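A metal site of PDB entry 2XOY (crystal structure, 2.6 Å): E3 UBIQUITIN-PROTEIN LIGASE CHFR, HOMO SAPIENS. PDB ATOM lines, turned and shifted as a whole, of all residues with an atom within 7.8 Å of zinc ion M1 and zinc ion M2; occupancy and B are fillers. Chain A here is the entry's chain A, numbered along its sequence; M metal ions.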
ATOM      1  N   ARG A  26      14.012  22.810  12.865  1.00  0.00           N
ATOM      2  CA  ARG A  26      13.691  24.240  12.828  1.00  0.00           C
ATOM      3  C   ARG A  26      12.194  24.563  12.706  1.00  0.00           C
ATOM      4  O   ARG A  26      11.738  25.593  13.199  1.00  0.00           O
ATOM      5  CB  ARG A  26      14.431  24.927  11.683  1.00  0.00           C
ATOM      6  CG  ARG A  26      15.902  25.186  11.941  1.00  0.00           C
ATOM      7  CD  ARG A  26      16.424  26.181  10.944  1.00  0.00           C
ATOM      8  NE  ARG A  26      17.488  25.645  10.111  1.00  0.00           N
ATOM      9  CZ  ARG A  26      17.834  26.134   8.922  1.00  0.00           C
ATOM     10  NH1 ARG A  26      17.166  27.174   8.425  1.00  0.00           N
ATOM     11  NH2 ARG A  26      18.818  25.585   8.223  1.00  0.00           N
ATOM     12  N   LEU A  81      17.227  13.931   6.370  1.00  0.00           N
ATOM     13  CA  LEU A  81      18.495  14.551   6.746  1.00  0.00           C
ATOM     14  C   LEU A  81      19.232  15.156   5.552  1.00  0.00           C
ATOM     15  O   LEU A  81      19.578  14.450   4.588  1.00  0.00           O
ATOM     16  CB  LEU A  81      19.390  13.560   7.489  1.00  0.00           C
ATOM     17  CG  LEU A  81      18.963  13.142   8.900  1.00  0.00           C
ATOM     18  CD1 LEU A  81      19.925  12.127   9.487  1.00  0.00           C
ATOM     19  CD2 LEU A  81      18.864  14.346   9.818  1.00  0.00           C
ATOM     20  N   CYS A  82      19.450  16.472   5.617  1.00  0.00           N
ATOM     21  CA  CYS A  82      20.246  17.144   4.601  1.00  0.00           C
ATOM     22  C   CYS A  82      21.534  16.373   4.488  1.00  0.00           C
ATOM     23  O   CYS A  82      22.184  16.108   5.487  1.00  0.00           O
ATOM     24  CB  CYS A  82      20.521  18.601   4.954  1.00  0.00           C
ATOM     25  SG  CYS A  82      21.629  19.418   3.787  1.00  0.00           S
ATOM     26  N   THR A  83      21.881  15.989   3.273  1.00  0.00           N
ATOM     27  CA  THR A  83      23.060  15.186   3.022  1.00  0.00           C
ATOM     28  C   THR A  83      24.337  15.966   3.323  1.00  0.00           C
ATOM     29  O   THR A  83      25.383  15.377   3.551  1.00  0.00           O
ATOM     30  CB  THR A  83      23.074  14.733   1.563  1.00  0.00           C
ATOM     31  OG1 THR A  83      21.898  13.945   1.312  1.00  0.00           O
ATOM     32  CG2 THR A  83      24.352  13.938   1.238  1.00  0.00           C
ATOM     33  N   CYS A  84      24.239  17.290   3.320  1.00  0.00           N
ATOM     34  CA  CYS A  84      25.424  18.128   3.447  1.00  0.00           C
ATOM     35  C   CYS A  84      25.631  18.540   4.881  1.00  0.00           C
ATOM     36  O   CYS A  84      26.705  18.334   5.444  1.00  0.00           O
ATOM     37  CB  CYS A  84      25.310  19.368   2.541  1.00  0.00           C
ATOM     38  SG  CYS A  84      26.278  20.806   3.123  1.00  0.00           S
ATOM     39  N   CYS A  85      24.606  19.135   5.464  1.00  0.00           N
ATOM     40  CA  CYS A  85      24.761  19.713   6.782  1.00  0.00           C
ATOM     41  C   CYS A  85      24.345  18.751   7.899  1.00  0.00           C
ATOM     42  O   CYS A  85      24.605  19.022   9.075  1.00  0.00           O
ATOM     43  CB  CYS A  85      23.987  21.026   6.877  1.00  0.00           C
ATOM     44  SG  CYS A  85      22.207  20.830   7.045  1.00  0.00           S
ATOM     45  N   PHE A  86      23.715  17.640   7.533  1.00  0.00           N
ATOM     46  CA  PHE A  86      23.352  16.571   8.470  1.00  0.00           C
ATOM     47  C   PHE A  86      22.128  16.853   9.360  1.00  0.00           C
ATOM     48  O   PHE A  86      21.677  15.968  10.091  1.00  0.00           O
ATOM     49  CB  PHE A  86      24.541  16.204   9.359  1.00  0.00           C
ATOM     50  CG  PHE A  86      25.744  15.714   8.599  1.00  0.00           C
ATOM     51  CD1 PHE A  86      25.597  14.785   7.572  1.00  0.00           C
ATOM     52  CD2 PHE A  86      27.018  16.173   8.904  1.00  0.00           C
ATOM     53  CE1 PHE A  86      26.703  14.323   6.881  1.00  0.00           C
ATOM     54  CE2 PHE A  86      28.124  15.711   8.213  1.00  0.00           C
ATOM     55  CZ  PHE A  86      27.967  14.791   7.190  1.00  0.00           C
ATOM     56  N   GLN A  87      21.591  18.059   9.290  1.00  0.00           N
ATOM     57  CA  GLN A  87      20.415  18.431  10.065  1.00  0.00           C
ATOM     58  C   GLN A  87      19.119  17.924   9.421  1.00  0.00           C
ATOM     59  O   GLN A  87      19.072  17.658   8.217  1.00  0.00           O
ATOM     60  CB  GLN A  87      20.347  19.946  10.233  1.00  0.00           C
ATOM     61  CG  GLN A  87      21.648  20.567  10.722  1.00  0.00           C
ATOM     62  CD  GLN A  87      22.091  20.036  12.080  1.00  0.00           C
ATOM     63  OE1 GLN A  87      21.459  20.326  13.106  1.00  0.00           O
ATOM     64  NE2 GLN A  87      23.172  19.267  12.096  1.00  0.00           N
ATOM     65  N   PRO A  88      18.063  17.789  10.238  1.00  0.00           N
ATOM     66  CA  PRO A  88      16.718  17.352   9.820  1.00  0.00           C
ATOM     67  C   PRO A  88      15.834  18.452   9.238  1.00  0.00           C
ATOM     68  O   PRO A  88      15.801  19.575   9.738  1.00  0.00           O
ATOM     69  CB  PRO A  88      16.096  16.882  11.127  1.00  0.00           C
ATOM     70  CG  PRO A  88      16.769  17.712  12.160  1.00  0.00           C
ATOM     71  CD  PRO A  88      18.186  17.822  11.703  1.00  0.00           C
ATOM     72  N   MET A  89      15.118  18.104   8.171  1.00  0.00           N
ATOM     73  CA  MET A  89      14.067  18.948   7.604  1.00  0.00           C
ATOM     74  C   MET A  89      12.841  18.069   7.414  1.00  0.00           C
ATOM     75  O   MET A  89      12.954  16.840   7.333  1.00  0.00           O
ATOM     76  CB  MET A  89      14.498  19.518   6.261  1.00  0.00           C
ATOM     77  CG  MET A  89      14.743  18.450   5.214  1.00  0.00           C
ATOM     78  SD  MET A  89      15.549  19.095   3.736  1.00  0.00           S
ATOM     79  CE  MET A  89      15.822  17.583   2.811  1.00  0.00           C
ATOM     80  N   PRO A 113      18.868  13.970  -0.493  1.00  0.00           N
ATOM     81  CA  PRO A 113      18.156  15.165  -0.025  1.00  0.00           C
ATOM     82  C   PRO A 113      19.092  16.252   0.504  1.00  0.00           C
ATOM     83  O   PRO A 113      20.137  15.946   1.099  1.00  0.00           O
ATOM     84  CB  PRO A 113      17.312  14.617   1.143  1.00  0.00           C
ATOM     85  CG  PRO A 113      17.775  13.178   1.346  1.00  0.00           C
ATOM     86  CD  PRO A 113      19.043  13.015   0.598  1.00  0.00           C
ATOM     87  N   PHE A 114      18.690  17.509   0.299  1.00  0.00           N
ATOM     88  CA  PHE A 114      19.509  18.654   0.690  1.00  0.00           C
ATOM     89  C   PHE A 114      18.613  19.788   1.104  1.00  0.00           C
ATOM     90  O   PHE A 114      17.568  20.000   0.499  1.00  0.00           O
ATOM     91  CB  PHE A 114      20.377  19.104  -0.494  1.00  0.00           C
ATOM     92  CG  PHE A 114      21.427  18.101  -0.895  1.00  0.00           C
ATOM     93  CD1 PHE A 114      22.707  18.181  -0.369  1.00  0.00           C
ATOM     94  CD2 PHE A 114      21.134  17.086  -1.785  1.00  0.00           C
ATOM     95  CE1 PHE A 114      23.682  17.285  -0.730  1.00  0.00           C
ATOM     96  CE2 PHE A 114      22.110  16.183  -2.153  1.00  0.00           C
ATOM     97  CZ  PHE A 114      23.392  16.284  -1.618  1.00  0.00           C
ATOM     98  N   CYS A 115      19.021  20.543   2.110  1.00  0.00           N
ATOM     99  CA  CYS A 115      18.137  21.533   2.724  1.00  0.00           C
ATOM    100  C   CYS A 115      18.218  22.900   2.086  1.00  0.00           C
ATOM    101  O   CYS A 115      17.321  23.728   2.262  1.00  0.00           O
ATOM    102  CB  CYS A 115      18.376  21.645   4.232  1.00  0.00           C
ATOM    103  SG  CYS A 115      19.827  22.630   4.739  1.00  0.00           S
ATOM    104  N   HIS A 116      19.290  23.155   1.339  1.00  0.00           N
ATOM    105  CA  HIS A 116      19.623  24.534   1.025  1.00  0.00           C
ATOM    106  C   HIS A 116      18.523  25.326   0.322  1.00  0.00           C
ATOM    107  O   HIS A 116      18.247  26.456   0.685  1.00  0.00           O
ATOM    108  CB  HIS A 116      20.890  24.622   0.201  1.00  0.00           C
ATOM    109  CG  HIS A 116      21.396  26.008   0.042  1.00  0.00           C
ATOM    110  ND1 HIS A 116      21.983  26.696   1.082  1.00  0.00           N
ATOM    111  CD2 HIS A 116      21.377  26.858  -1.011  1.00  0.00           C
ATOM    112  CE1 HIS A 116      22.320  27.904   0.665  1.00  0.00           C
ATOM    113  NE2 HIS A 116      21.963  28.025  -0.608  1.00  0.00           N
ATOM    114  N   LEU A 117      17.897  24.729  -0.669  1.00  0.00           N
ATOM    115  CA  LEU A 117      16.839  25.410  -1.388  1.00  0.00           C
ATOM    116  C   LEU A 117      15.575  25.490  -0.566  1.00  0.00           C
ATOM    117  O   LEU A 117      14.785  26.422  -0.725  1.00  0.00           O
ATOM    118  CB  LEU A 117      16.551  24.727  -2.725  1.00  0.00           C
ATOM    119  CG  LEU A 117      17.461  25.134  -3.878  1.00  0.00           C
ATOM    120  CD1 LEU A 117      17.113  24.342  -5.113  1.00  0.00           C
ATOM    121  CD2 LEU A 117      17.354  26.651  -4.138  1.00  0.00           C
ATOM    122  N   TRP A 119      15.209  25.836   2.970  1.00  0.00           N
ATOM    123  CA  TRP A 119      15.300  26.887   4.001  1.00  0.00           C
ATOM    124  C   TRP A 119      16.704  27.421   4.284  1.00  0.00           C
ATOM    125  O   TRP A 119      16.919  28.049   5.323  1.00  0.00           O
ATOM    126  CB  TRP A 119      14.664  26.419   5.317  1.00  0.00           C
ATOM    127  CG  TRP A 119      15.342  25.221   5.957  1.00  0.00           C
ATOM    128  CD1 TRP A 119      16.569  24.720   5.658  1.00  0.00           C
ATOM    129  CD2 TRP A 119      14.813  24.402   7.010  1.00  0.00           C
ATOM    130  NE1 TRP A 119      16.835  23.626   6.454  1.00  0.00           N
ATOM    131  CE2 TRP A 119      15.780  23.408   7.293  1.00  0.00           C
ATOM    132  CE3 TRP A 119      13.624  24.402   7.754  1.00  0.00           C
ATOM    133  CZ2 TRP A 119      15.583  22.428   8.270  1.00  0.00           C
ATOM    134  CZ3 TRP A 119      13.435  23.436   8.719  1.00  0.00           C
ATOM    135  CH2 TRP A 119      14.407  22.458   8.974  1.00  0.00           C
ATOM    136  N   GLY A 120      17.652  27.158   3.404  1.00  0.00           N
ATOM    137  CA  GLY A 120      19.027  27.639   3.583  1.00  0.00           C
ATOM    138  C   GLY A 120      19.909  26.779   4.477  1.00  0.00           C
ATOM    139  O   GLY A 120      19.690  26.652   5.683  1.00  0.00           O
ATOM    140  N   CYS A 121      20.935  26.194   3.872  1.00  0.00           N
ATOM    141  CA  CYS A 121      21.880  25.355   4.594  1.00  0.00           C
ATOM    142  C   CYS A 121      23.034  26.187   5.181  1.00  0.00           C
ATOM    143  O   CYS A 121      23.342  27.272   4.696  1.00  0.00           O
ATOM    144  CB  CYS A 121      22.437  24.289   3.660  1.00  0.00           C
ATOM    145  SG  CYS A 121      23.584  23.137   4.410  1.00  0.00           S
ATOM    146  N   THR A 122      23.668  25.658   6.228  1.00  0.00           N
ATOM    147  CA  THR A 122      24.854  26.302   6.800  1.00  0.00           C
ATOM    148  C   THR A 122      25.854  25.323   7.373  1.00  0.00           C
ATOM    149  O   THR A 122      25.559  24.561   8.300  1.00  0.00           O
ATOM    150  CB  THR A 122      24.489  27.309   7.910  1.00  0.00           C
ATOM    151  OG1 THR A 122      24.049  28.536   7.307  1.00  0.00           O
ATOM    152  CG2 THR A 122      25.719  27.602   8.766  1.00  0.00           C
ATOM    153  N   ARG A 123      27.054  25.356   6.818  1.00  0.00           N
ATOM    154  CA  ARG A 123      28.140  24.511   7.269  1.00  0.00           C
ATOM    155  C   ARG A 123      29.403  25.051   6.632  1.00  0.00           C
ATOM    156  O   ARG A 123      29.362  25.667   5.555  1.00  0.00           O
ATOM    157  CB  ARG A 123      27.904  23.060   6.849  1.00  0.00           C
ATOM    158  CG  ARG A 123      28.933  22.077   7.402  1.00  0.00           C
ATOM    159  CD  ARG A 123      28.608  20.642   7.022  1.00  0.00           C
ATOM    160  NE  ARG A 123      28.768  20.436   5.591  1.00  0.00           N
ATOM    161  CZ  ARG A 123      29.850  19.890   5.040  1.00  0.00           C
ATOM    162  NH1 ARG A 123      30.861  19.492   5.794  1.00  0.00           N
ATOM    163  NH2 ARG A 123      29.917  19.744   3.718  1.00  0.00           N
ATOM    164  N   GLY A 125      32.210  25.018   4.386  1.00  0.00           N
ATOM    165  CA  GLY A 125      32.516  24.285   3.168  1.00  0.00           C
ATOM    166  C   GLY A 125      31.282  24.140   2.315  1.00  0.00           C
ATOM    167  O   GLY A 125      31.358  23.731   1.150  1.00  0.00           O
ATOM    168  N   CYS A 126      30.129  24.465   2.892  1.00  0.00           N
ATOM    169  CA  CYS A 126      28.905  24.482   2.124  1.00  0.00           C
ATOM    170  C   CYS A 126      28.790  25.821   1.427  1.00  0.00           C
ATOM    171  O   CYS A 126      28.586  26.849   2.068  1.00  0.00           O
ATOM    172  CB  CYS A 126      27.667  24.227   3.009  1.00  0.00           C
ATOM    173  SG  CYS A 126      26.099  24.386   2.089  1.00  0.00           S
ATOM    174  N   TYR A 127      28.927  25.799   0.100  1.00  0.00           N
ATOM    175  CA  TYR A 127      28.838  27.002  -0.728  1.00  0.00           C
ATOM    176  C   TYR A 127      27.392  27.343  -1.104  1.00  0.00           C
ATOM    177  O   TYR A 127      27.143  28.377  -1.734  1.00  0.00           O
ATOM    178  CB  TYR A 127      29.633  26.785  -1.999  1.00  0.00           C
ATOM    179  CG  TYR A 127      31.058  26.310  -1.804  1.00  0.00           C
ATOM    180  CD1 TYR A 127      31.926  26.971  -0.956  1.00  0.00           C
ATOM    181  CD2 TYR A 127      31.547  25.217  -2.506  1.00  0.00           C
ATOM    182  CE1 TYR A 127      33.231  26.548  -0.785  1.00  0.00           C
ATOM    183  CE2 TYR A 127      32.835  24.792  -2.350  1.00  0.00           C
ATOM    184  CZ  TYR A 127      33.676  25.451  -1.491  1.00  0.00           C
ATOM    185  OH  TYR A 127      34.983  25.015  -1.335  1.00  0.00           O
ATOM    186  N   GLY A 128      26.461  26.466  -0.723  1.00  0.00           N
ATOM    187  CA  GLY A 128      25.106  26.436  -1.278  1.00  0.00           C
ATOM    188  C   GLY A 128      24.902  25.093  -1.980  1.00  0.00           C
ATOM    189  O   GLY A 128      25.135  24.959  -3.181  1.00  0.00           O
ATOM    190  N   CYS A 129      24.466  24.086  -1.232  1.00  0.00           N
ATOM    191  CA  CYS A 129      24.534  22.695  -1.702  1.00  0.00           C
ATOM    192  C   CYS A 129      23.447  22.261  -2.679  1.00  0.00           C
ATOM    193  O   CYS A 129      23.404  21.099  -3.074  1.00  0.00           O
ATOM    194  CB  CYS A 129      24.609  21.722  -0.514  1.00  0.00           C
ATOM    195  SG  CYS A 129      23.375  21.990   0.807  1.00  0.00           S
ATOM    196  N   LEU A 130      22.553  23.171  -3.065  1.00  0.00           N
ATOM    197  CA  LEU A 130      21.544  22.847  -4.076  1.00  0.00           C
ATOM    198  C   LEU A 130      21.156  24.066  -4.895  1.00  0.00           C
ATOM    199  O   LEU A 130      20.829  25.119  -4.349  1.00  0.00           O
ATOM    200  CB  LEU A 130      20.306  22.185  -3.447  1.00  0.00           C
ATOM    201  CG  LEU A 130      19.400  21.325  -4.339  1.00  0.00           C
ATOM    202  CD1 LEU A 130      20.017  19.946  -4.615  1.00  0.00           C
ATOM    203  CD2 LEU A 130      17.979  21.179  -3.755  1.00  0.00           C
ATOM    204  N   TYR A 199      26.069  19.964  -5.011  1.00  0.00           N
ATOM    205  CA  TYR A 199      27.442  20.368  -5.157  1.00  0.00           C
ATOM    206  C   TYR A 199      28.229  19.265  -5.859  1.00  0.00           C
ATOM    207  O   TYR A 199      28.906  19.539  -6.858  1.00  0.00           O
ATOM    208  CB  TYR A 199      28.077  20.735  -3.793  1.00  0.00           C
ATOM    209  CG  TYR A 199      29.587  20.814  -3.869  1.00  0.00           C
ATOM    210  CD1 TYR A 199      30.230  21.874  -4.485  1.00  0.00           C
ATOM    211  CD2 TYR A 199      30.379  19.812  -3.321  1.00  0.00           C
ATOM    212  CE1 TYR A 199      31.602  21.934  -4.564  1.00  0.00           C
ATOM    213  CE2 TYR A 199      31.756  19.863  -3.390  1.00  0.00           C
ATOM    214  CZ  TYR A 199      32.360  20.919  -4.022  1.00  0.00           C
ATOM    215  OH  TYR A 199      33.742  20.976  -4.097  1.00  0.00           O
HETATM  216 ZN    ZN M   1      21.646  21.420   4.830  1.00  0.00          ZN
HETATM  217 ZN    ZN M   2      24.775  22.395   2.507  1.00  0.00          ZN
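SG of Cys 115 sits close to NE1 of Trp 119, 3.6 Å away. The backbone NH (N) of Tyr 199 lies within hydrogen-bond range of the backbone carbonyl oxygen (O) of Cys 129 (3.5 Å). The side-chain sulfur (SG) of Cys 82 sits close to the backbone NH (N) of Cys 84 (3.4 Å). N of Cys 82 sits at hydrogen-bond distance from O of Gln 87 (2.9 Å). NE of Arg 123 lies within hydrogen-bond range of O of Cys 84, at 2.9 Å. The backbone carbonyl oxygen (O) of Cys 85 lies within hydrogen-bond range of the side-chain amide nitrogen (NE2) of Gln 87 (3.4 Å). N of Cys 121 is in hydrogen-bond range of ND1 of His 116, at 3.0 Å. SG of Cys 126 lies close to N of Gly 128, 3.5 Å away.
Four residues have an atom within 4 Å of zinc ion M1: Cys 82, Cys 85, Cys 115 and Cys 121. The nearest printed residue that does not touch zinc ion M1 is Cys 129 (4.4 Å).
The nearest printed residue that does not touch zinc ion M2 is Cys 85 (4.4 Å).
Zinc ion M1 is bound by the side-chain sulfur of Cys 115 (2.2 Å), the side-chain sulfur of Cys 82 (2.3 Å), the side-chain sulfur of Cys 85 (2.4 Å) and the side-chain sulfur of Cys 121 (2.6 Å).
Zinc ion M2 is bound by SG of Cys 129 (2.2 Å), SG of Cys 84 (2.3 Å), SG of Cys 121 (2.4 Å) and SG of Cys 126 (2.4 Å). Zinc ion M2 has four donor atoms within binding distance.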
